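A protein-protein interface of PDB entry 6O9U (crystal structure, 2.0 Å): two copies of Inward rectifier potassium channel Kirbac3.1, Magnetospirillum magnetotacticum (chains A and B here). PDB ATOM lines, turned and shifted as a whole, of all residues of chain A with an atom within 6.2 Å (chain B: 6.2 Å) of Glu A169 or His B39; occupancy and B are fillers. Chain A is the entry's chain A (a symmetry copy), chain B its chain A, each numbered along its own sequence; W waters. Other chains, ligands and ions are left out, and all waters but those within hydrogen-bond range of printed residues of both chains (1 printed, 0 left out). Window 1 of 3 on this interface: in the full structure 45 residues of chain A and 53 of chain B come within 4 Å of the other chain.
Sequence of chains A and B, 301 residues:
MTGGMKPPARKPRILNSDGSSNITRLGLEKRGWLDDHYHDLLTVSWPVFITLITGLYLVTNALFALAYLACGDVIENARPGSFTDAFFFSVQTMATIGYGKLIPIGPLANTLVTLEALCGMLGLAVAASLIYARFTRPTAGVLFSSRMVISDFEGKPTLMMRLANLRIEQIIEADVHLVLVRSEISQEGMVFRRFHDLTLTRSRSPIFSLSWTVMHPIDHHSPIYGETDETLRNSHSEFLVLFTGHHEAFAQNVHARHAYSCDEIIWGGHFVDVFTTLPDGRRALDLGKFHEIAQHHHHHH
Water W1 lies within hydrogen-bond range of NH1 of Arg B25 and O of Ile A168.
The backbone carbonyl oxygen (O) of Asn A165 is in hydrogen-bond range of the guanidinium group (NH2) of Arg B25 (2.6 Å). NH1 of Arg B25 is in hydrogen-bond range of O of Arg A167, at 2.8 Å. The guanidinium group (NE) of Arg A167 lies within salt-bridge range of the side-chain carboxylate (OD2) of Asp B36 (2.8 Å). The side-chain carboxylate (OE1) of Glu A169 sits at hydrogen-bond distance from a ring nitrogen (NE2) of His B39 (2.6 Å). The guanidinium group (NH1) of Arg B137 sits at hydrogen-bond distance from the backbone carbonyl oxygen (O) of Ala A249, 2.8 Å away.
Of the 12 printed residues of chain A, 5 touch a printed residue of chain B. Among the printed residues, 13 pairs touch across the chains. Among the printed residues, Asp or Glu carboxylates within 4 Å of a Lys or Arg side-chain nitrogen of the other chain: Arg A167 with Asp B36 (2.8 Å).
No position is printed for both chains. Of the 13 pairs that touch across the chains among the printed residues, none has its exchanged pair printed and touching as well.
Printed residues of chain B within 4 Å of Glu A169: His B39 (2.6 Å) and Thr B43 (3.6 Å). His B39 touches just these residues of chain A: Arg A167 (3.5 Å), Glu A169 (2.6 Å), Ala A249 (3.6 Å) and Phe A250 (3.8 Å). Printed residues of chain B within 4 Å of Asn A165: Arg B25. Printed residues of chain A within 4 Å of Thr B43: Glu A169 and Ala A249. Of the printed residues of chain A, Arg B25 touches Asn A165 and Arg A167. Printed residues of chain A within 4 Å of Asp B36: Arg A167. Of the printed residues of chain A, Tyr B38 touches Phe A250. Ile A171 touches none of the printed residues of chain B. His A247 touches none of the printed residues of chain B. The nearest residue of chain B that does not touch Glu A169 is Arg B25 (5.9 Å).
Among the printed residues, merely in contact across the chains: Arg A167 with His B39 (3.5 Å), Glu A169 with Thr B43 (3.6 Å), Ala A249 with His B39 (3.6 Å), Ala A249 with Thr B43 (3.99 Å), Phe A250 with Tyr B38 (3.6 Å), Phe A250 with His B39 (3.8 Å), Phe A250 with Leu B42 (3.6 Å) and Phe A250 with Arg B137 (3.9 Å).
The side-chain carboxylate of Asp B36 lies close to a ring nitrogen (ND1) of His B39, at 3.5 Å. ND1 of His B39 is in hydrogen-bond range of OD1 of Asp B40 (2.7 Å). OG1 of Thr B43 is in hydrogen-bond range of O of His B39. OD1 of Asn A165 sits at hydrogen-bond distance from N of Arg A167. O of Glu A169 lies within hydrogen-bond range of ND2 of Asn A165, at 2.8 Å. The backbone NH of Ala A249 is in hydrogen-bond range of a ring nitrogen (ND1) of His A247 (3.1 Å).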
ATOM      1  N   ASN A 165       5.114  -5.757   8.384  1.00  0.00           N
ATOM      2  CA  ASN A 165       4.128  -4.690   8.486  1.00  0.00           C
ATOM      3  C   ASN A 165       4.674  -3.608   9.410  1.00  0.00           C
ATOM      4  O   ASN A 165       5.007  -3.884  10.565  1.00  0.00           O
ATOM      5  CB  ASN A 165       2.807  -5.237   9.024  1.00  0.00           C
ATOM      6  CG  ASN A 165       1.675  -4.238   8.926  1.00  0.00           C
ATOM      7  OD1 ASN A 165       1.890  -3.067   8.607  1.00  0.00           O
ATOM      8  ND2 ASN A 165       0.459  -4.694   9.206  1.00  0.00           N
ATOM      9  N   ARG A 167       2.911  -0.923  10.272  1.00  0.00           N
ATOM     10  CA  ARG A 167       1.788  -0.290  10.943  1.00  0.00           C
ATOM     11  C   ARG A 167       1.115  -1.299  11.864  1.00  0.00           C
ATOM     12  O   ARG A 167       1.364  -2.505  11.794  1.00  0.00           O
ATOM     13  CB  ARG A 167       0.786   0.265   9.927  1.00  0.00           C
ATOM     14  CG  ARG A 167       1.373   1.292   8.976  1.00  0.00           C
ATOM     15  CD  ARG A 167       0.323   1.769   8.005  1.00  0.00           C
ATOM     16  NE  ARG A 167       0.760   2.911   7.205  1.00  0.00           N
ATOM     17  CZ  ARG A 167       0.663   3.002   5.881  1.00  0.00           C
ATOM     18  NH1 ARG A 167       0.131   2.023   5.161  1.00  0.00           N
ATOM     19  NH2 ARG A 167       1.093   4.096   5.268  1.00  0.00           N
ATOM     20  N   ILE A 168       0.250  -0.787  12.740  1.00  0.00           N
ATOM     21  CA  ILE A 168      -0.429  -1.644  13.708  1.00  0.00           C
ATOM     22  C   ILE A 168      -1.712  -2.255  13.154  1.00  0.00           C
ATOM     23  O   ILE A 168      -2.161  -3.290  13.667  1.00  0.00           O
ATOM     24  CB  ILE A 168      -0.738  -0.875  15.006  1.00  0.00           C
ATOM     25  CG1 ILE A 168      -1.665   0.312  14.732  1.00  0.00           C
ATOM     26  CG2 ILE A 168       0.565  -0.411  15.653  1.00  0.00           C
ATOM     27  CD1 ILE A 168      -2.118   1.046  15.975  1.00  0.00           C
ATOM     28  N   GLU A 169      -2.312  -1.654  12.129  1.00  0.00           N
ATOM     29  CA  GLU A 169      -3.479  -2.247  11.495  1.00  0.00           C
ATOM     30  C   GLU A 169      -3.047  -3.345  10.522  1.00  0.00           C
ATOM     31  O   GLU A 169      -1.923  -3.354  10.011  1.00  0.00           O
ATOM     32  CB  GLU A 169      -4.309  -1.188  10.764  1.00  0.00           C
ATOM     33  CG  GLU A 169      -4.757  -0.018  11.638  1.00  0.00           C
ATOM     34  CD  GLU A 169      -3.719   1.084  11.742  1.00  0.00           C
ATOM     35  OE1 GLU A 169      -2.768   1.088  10.936  1.00  0.00           O
ATOM     36  OE2 GLU A 169      -3.857   1.951  12.633  1.00  0.00           O
ATOM     37  N   GLN A 170      -3.963  -4.272  10.267  1.00  0.00           N
ATOM     38  CA  GLN A 170      -3.684  -5.458   9.472  1.00  0.00           C
ATOM     39  C   GLN A 170      -4.155  -5.271   8.033  1.00  0.00           C
ATOM     40  O   GLN A 170      -4.926  -4.361   7.717  1.00  0.00           O
ATOM     41  CB  GLN A 170      -4.358  -6.684  10.098  1.00  0.00           C
ATOM     42  CG  GLN A 170      -3.836  -7.021  11.493  1.00  0.00           C
ATOM     43  CD  GLN A 170      -4.687  -8.052  12.211  1.00  0.00           C
ATOM     44  OE1 GLN A 170      -5.913  -8.040  12.110  1.00  0.00           O
ATOM     45  NE2 GLN A 170      -4.042  -8.951  12.941  1.00  0.00           N
ATOM     46  N   ILE A 171      -3.668  -6.147   7.156  1.00  0.00           N
ATOM     47  CA  ILE A 171      -3.981  -6.104   5.733  1.00  0.00           C
ATOM     48  C   ILE A 171      -4.715  -7.387   5.366  1.00  0.00           C
ATOM     49  O   ILE A 171      -4.221  -8.491   5.629  1.00  0.00           O
ATOM     50  CB  ILE A 171      -2.715  -5.910   4.881  1.00  0.00           C
ATOM     51  CG1 ILE A 171      -1.954  -4.670   5.376  1.00  0.00           C
ATOM     52  CG2 ILE A 171      -3.091  -5.750   3.417  1.00  0.00           C
ATOM     53  CD1 ILE A 171      -0.686  -4.335   4.610  1.00  0.00           C
ATOM     54  N   PHE A 208      -2.670 -10.501   6.833  1.00  0.00           N
ATOM     55  CA  PHE A 208      -1.267 -10.175   7.047  1.00  0.00           C
ATOM     56  C   PHE A 208      -1.174  -9.215   8.227  1.00  0.00           C
ATOM     57  O   PHE A 208      -1.768  -8.132   8.200  1.00  0.00           O
ATOM     58  CB  PHE A 208      -0.672  -9.566   5.779  1.00  0.00           C
ATOM     59  CG  PHE A 208       0.720  -9.036   5.949  1.00  0.00           C
ATOM     60  CD1 PHE A 208       1.787  -9.896   6.148  1.00  0.00           C
ATOM     61  CD2 PHE A 208       0.967  -7.675   5.889  1.00  0.00           C
ATOM     62  CE1 PHE A 208       3.070  -9.407   6.298  1.00  0.00           C
ATOM     63  CE2 PHE A 208       2.249  -7.182   6.036  1.00  0.00           C
ATOM     64  CZ  PHE A 208       3.300  -8.049   6.239  1.00  0.00           C
ATOM     65  N   SER A 209      -0.428  -9.610   9.259  1.00  0.00           N
ATOM     66  CA  SER A 209      -0.391  -8.872  10.518  1.00  0.00           C
ATOM     67  C   SER A 209       0.983  -8.290  10.814  1.00  0.00           C
ATOM     68  O   SER A 209       1.107  -7.070  10.963  1.00  0.00           O
ATOM     69  CB  SER A 209      -0.844  -9.788  11.663  1.00  0.00           C
ATOM     70  OG  SER A 209      -2.169 -10.241  11.459  1.00  0.00           O
ATOM     71  N   HIS A 247      -6.135  -2.762   3.055  1.00  0.00           N
ATOM     72  CA  HIS A 247      -5.584  -2.231   4.295  1.00  0.00           C
ATOM     73  C   HIS A 247      -6.706  -1.727   5.199  1.00  0.00           C
ATOM     74  O   HIS A 247      -7.520  -0.890   4.789  1.00  0.00           O
ATOM     75  CB  HIS A 247      -4.582  -1.119   4.000  1.00  0.00           C
ATOM     76  CG  HIS A 247      -3.607  -0.888   5.108  1.00  0.00           C
ATOM     77  ND1 HIS A 247      -3.993  -0.459   6.358  1.00  0.00           N
ATOM     78  CD2 HIS A 247      -2.262  -1.046   5.165  1.00  0.00           C
ATOM     79  CE1 HIS A 247      -2.931  -0.355   7.135  1.00  0.00           C
ATOM     80  NE2 HIS A 247      -1.868  -0.705   6.434  1.00  0.00           N
ATOM     81  N   GLU A 248      -6.738  -2.232   6.436  1.00  0.00           N
ATOM     82  CA  GLU A 248      -7.784  -1.859   7.384  1.00  0.00           C
ATOM     83  C   GLU A 248      -7.809  -0.362   7.653  1.00  0.00           C
ATOM     84  O   GLU A 248      -8.882   0.228   7.817  1.00  0.00           O
ATOM     85  CB  GLU A 248      -7.583  -2.600   8.702  1.00  0.00           C
ATOM     86  CG  GLU A 248      -8.034  -4.022   8.688  1.00  0.00           C
ATOM     87  CD  GLU A 248      -8.218  -4.565  10.086  1.00  0.00           C
ATOM     88  OE1 GLU A 248      -7.553  -4.051  11.012  1.00  0.00           O
ATOM     89  OE2 GLU A 248      -9.021  -5.504  10.262  1.00  0.00           O
ATOM     90  N   ALA A 249      -6.634   0.264   7.741  1.00  0.00           N
ATOM     91  CA  ALA A 249      -6.572   1.673   8.113  1.00  0.00           C
ATOM     92  C   ALA A 249      -7.295   2.558   7.111  1.00  0.00           C
ATOM     93  O   ALA A 249      -7.793   3.629   7.477  1.00  0.00           O
ATOM     94  CB  ALA A 249      -5.115   2.114   8.254  1.00  0.00           C
ATOM     95  N   PHE A 250      -7.369   2.134   5.846  1.00  0.00           N
ATOM     96  CA  PHE A 250      -7.927   2.956   4.784  1.00  0.00           C
ATOM     97  C   PHE A 250      -9.194   2.394   4.158  1.00  0.00           C
ATOM     98  O   PHE A 250      -9.882   3.128   3.436  1.00  0.00           O
ATOM     99  CB  PHE A 250      -6.885   3.156   3.670  1.00  0.00           C
ATOM    100  CG  PHE A 250      -5.552   3.632   4.167  1.00  0.00           C
ATOM    101  CD1 PHE A 250      -5.342   4.972   4.446  1.00  0.00           C
ATOM    102  CD2 PHE A 250      -4.508   2.743   4.349  1.00  0.00           C
ATOM    103  CE1 PHE A 250      -4.114   5.416   4.905  1.00  0.00           C
ATOM    104  CE2 PHE A 250      -3.278   3.179   4.807  1.00  0.00           C
ATOM    105  CZ  PHE A 250      -3.081   4.521   5.085  1.00  0.00           C
ATOM    106  N   ARG B  25       5.373  -5.916  20.106  1.00  0.00           N
ATOM    107  CA  ARG B  25       6.147  -5.355  19.002  1.00  0.00           C
ATOM    108  C   ARG B  25       7.270  -4.508  19.584  1.00  0.00           C
ATOM    109  O   ARG B  25       7.058  -3.361  19.986  1.00  0.00           O
ATOM    110  CB  ARG B  25       5.251  -4.539  18.079  1.00  0.00           C
ATOM    111  CG  ARG B  25       4.167  -5.364  17.394  1.00  0.00           C
ATOM    112  CD  ARG B  25       3.528  -4.628  16.222  1.00  0.00           C
ATOM    113  NE  ARG B  25       4.515  -4.204  15.234  1.00  0.00           N
ATOM    114  CZ  ARG B  25       4.236  -3.886  13.973  1.00  0.00           C
ATOM    115  NH1 ARG B  25       2.990  -3.951  13.520  1.00  0.00           N
ATOM    116  NH2 ARG B  25       5.214  -3.510  13.158  1.00  0.00           N
ATOM    117  N   ASP B  36       4.180   9.227   8.878  1.00  0.00           N
ATOM    118  CA  ASP B  36       3.064   8.483   8.305  1.00  0.00           C
ATOM    119  C   ASP B  36       1.801   9.333   8.440  1.00  0.00           C
ATOM    120  O   ASP B  36       0.772   8.890   8.954  1.00  0.00           O
ATOM    121  CB  ASP B  36       2.919   7.128   9.001  1.00  0.00           C
ATOM    122  CG  ASP B  36       2.284   6.071   8.117  1.00  0.00           C
ATOM    123  OD1 ASP B  36       2.172   6.288   6.892  1.00  0.00           O
ATOM    124  OD2 ASP B  36       1.898   5.013   8.656  1.00  0.00           O
ATOM    125  N   HIS B  37       1.871  10.579   7.961  1.00  0.00           N
ATOM    126  CA  HIS B  37       0.910  11.592   8.391  1.00  0.00           C
ATOM    127  C   HIS B  37      -0.493  11.306   7.871  1.00  0.00           C
ATOM    128  O   HIS B  37      -1.471  11.459   8.613  1.00  0.00           O
ATOM    129  CB  HIS B  37       1.377  12.989   7.966  1.00  0.00           C
ATOM    130  CG  HIS B  37       1.735  13.107   6.516  1.00  0.00           C
ATOM    131  ND1 HIS B  37       0.790  13.163   5.515  1.00  0.00           N
ATOM    132  CD2 HIS B  37       2.938  13.204   5.904  1.00  0.00           C
ATOM    133  CE1 HIS B  37       1.396  13.275   4.346  1.00  0.00           C
ATOM    134  NE2 HIS B  37       2.700  13.304   4.554  1.00  0.00           N
ATOM    135  N   TYR B  38      -0.627  10.901   6.607  1.00  0.00           N
ATOM    136  CA  TYR B  38      -1.957  10.611   6.081  1.00  0.00           C
ATOM    137  C   TYR B  38      -2.608   9.481   6.869  1.00  0.00           C
ATOM    138  O   TYR B  38      -3.750   9.604   7.328  1.00  0.00           O
ATOM    139  CB  TYR B  38      -1.881  10.266   4.592  1.00  0.00           C
ATOM    140  CG  TYR B  38      -3.235   9.987   3.975  1.00  0.00           C
ATOM    141  CD1 TYR B  38      -4.188  10.990   3.867  1.00  0.00           C
ATOM    142  CD2 TYR B  38      -3.561   8.719   3.508  1.00  0.00           C
ATOM    143  CE1 TYR B  38      -5.427  10.743   3.310  1.00  0.00           C
ATOM    144  CE2 TYR B  38      -4.800   8.461   2.948  1.00  0.00           C
ATOM    145  CZ  TYR B  38      -5.727   9.477   2.852  1.00  0.00           C
ATOM    146  OH  TYR B  38      -6.961   9.228   2.299  1.00  0.00           O
ATOM    147  N   HIS B  39      -1.883   8.373   7.046  1.00  0.00           N
ATOM    148  CA  HIS B  39      -2.373   7.271   7.868  1.00  0.00           C
ATOM    149  C   HIS B  39      -2.781   7.750   9.255  1.00  0.00           C
ATOM    150  O   HIS B  39      -3.844   7.381   9.768  1.00  0.00           O
ATOM    151  CB  HIS B  39      -1.295   6.192   7.977  1.00  0.00           C
ATOM    152  CG  HIS B  39      -1.523   5.219   9.092  1.00  0.00           C
ATOM    153  ND1 HIS B  39      -1.110   5.458  10.384  1.00  0.00           N
ATOM    154  CD2 HIS B  39      -2.120   4.004   9.107  1.00  0.00           C
ATOM    155  CE1 HIS B  39      -1.441   4.432  11.147  1.00  0.00           C
ATOM    156  NE2 HIS B  39      -2.055   3.536  10.396  1.00  0.00           N
ATOM    157  N   ASP B  40      -1.938   8.569   9.886  1.00  0.00           N
ATOM    158  CA  ASP B  40      -2.200   8.976  11.263  1.00  0.00           C
ATOM    159  C   ASP B  40      -3.411   9.899  11.351  1.00  0.00           C
ATOM    160  O   ASP B  40      -4.185   9.821  12.311  1.00  0.00           O
ATOM    161  CB  ASP B  40      -0.960   9.649  11.852  1.00  0.00           C
ATOM    162  CG  ASP B  40       0.201   8.680  12.029  1.00  0.00           C
ATOM    163  OD1 ASP B  40      -0.010   7.459  11.866  1.00  0.00           O
ATOM    164  OD2 ASP B  40       1.324   9.140  12.327  1.00  0.00           O
ATOM    165  N   LEU B  41      -3.594  10.775  10.360  1.00  0.00           N
ATOM    166  CA  LEU B  41      -4.774  11.632  10.348  1.00  0.00           C
ATOM    167  C   LEU B  41      -6.059  10.818  10.284  1.00  0.00           C
ATOM    168  O   LEU B  41      -7.088  11.244  10.821  1.00  0.00           O
ATOM    169  CB  LEU B  41      -4.709  12.601   9.168  1.00  0.00           C
ATOM    170  CG  LEU B  41      -3.645  13.695   9.265  1.00  0.00           C
ATOM    171  CD1 LEU B  41      -3.461  14.372   7.917  1.00  0.00           C
ATOM    172  CD2 LEU B  41      -4.014  14.717  10.330  1.00  0.00           C
ATOM    173  N   LEU B  42      -6.022   9.649   9.642  1.00  0.00           N
ATOM    174  CA  LEU B  42      -7.209   8.812   9.522  1.00  0.00           C
ATOM    175  C   LEU B  42      -7.421   7.886  10.712  1.00  0.00           C
ATOM    176  O   LEU B  42      -8.535   7.379  10.884  1.00  0.00           O
ATOM    177  CB  LEU B  42      -7.136   7.956   8.253  1.00  0.00           C
ATOM    178  CG  LEU B  42      -7.030   8.673   6.904  1.00  0.00           C
ATOM    179  CD1 LEU B  42      -7.298   7.685   5.785  1.00  0.00           C
ATOM    180  CD2 LEU B  42      -7.978   9.855   6.805  1.00  0.00           C
ATOM    181  N   THR B  43      -6.395   7.652  11.532  1.00  0.00           N
ATOM    182  CA  THR B  43      -6.478   6.646  12.581  1.00  0.00           C
ATOM    183  C   THR B  43      -6.454   7.216  13.993  1.00  0.00           C
ATOM    184  O   THR B  43      -6.796   6.491  14.932  1.00  0.00           O
ATOM    185  CB  THR B  43      -5.343   5.620  12.429  1.00  0.00           C
ATOM    186  OG1 THR B  43      -4.079   6.290  12.365  1.00  0.00           O
ATOM    187  CG2 THR B  43      -5.542   4.801  11.166  1.00  0.00           C
ATOM    188  N   VAL B  44      -6.070   8.482  14.178  1.00  0.00           N
ATOM    189  CA  VAL B  44      -6.229   9.089  15.494  1.00  0.00           C
ATOM    190  C   VAL B  44      -7.715   9.142  15.844  1.00  0.00           C
ATOM    191  O   VAL B  44      -8.594   9.092  14.974  1.00  0.00           O
ATOM    192  CB  VAL B  44      -5.609  10.494  15.571  1.00  0.00           C
ATOM    193  CG1 VAL B  44      -4.093  10.422  15.475  1.00  0.00           C
ATOM    194  CG2 VAL B  44      -6.191  11.410  14.492  1.00  0.00           C
ATOM    195  N   ARG B 137     -15.287   3.752   5.930  1.00  0.00           N
ATOM    196  CA  ARG B 137     -14.600   2.544   6.381  1.00  0.00           C
ATOM    197  C   ARG B 137     -15.605   1.738   7.192  1.00  0.00           C
ATOM    198  O   ARG B 137     -15.449   1.557   8.406  1.00  0.00           O
ATOM    199  CB  ARG B 137     -13.352   2.895   7.191  1.00  0.00           C
ATOM    200  CG  ARG B 137     -12.373   3.785   6.427  1.00  0.00           C
ATOM    201  CD  ARG B 137     -11.164   4.149   7.267  1.00  0.00           C
ATOM    202  NE  ARG B 137     -11.517   5.042   8.366  1.00  0.00           N
ATOM    203  CZ  ARG B 137     -10.683   5.409   9.333  1.00  0.00           C
ATOM    204  NH1 ARG B 137      -9.436   4.956   9.351  1.00  0.00           N
ATOM    205  NH2 ARG B 137     -11.098   6.228  10.291  1.00  0.00           N
HETATM  206  O   HOH W   1       0.589  -4.749  15.037  1.00  0.00           O
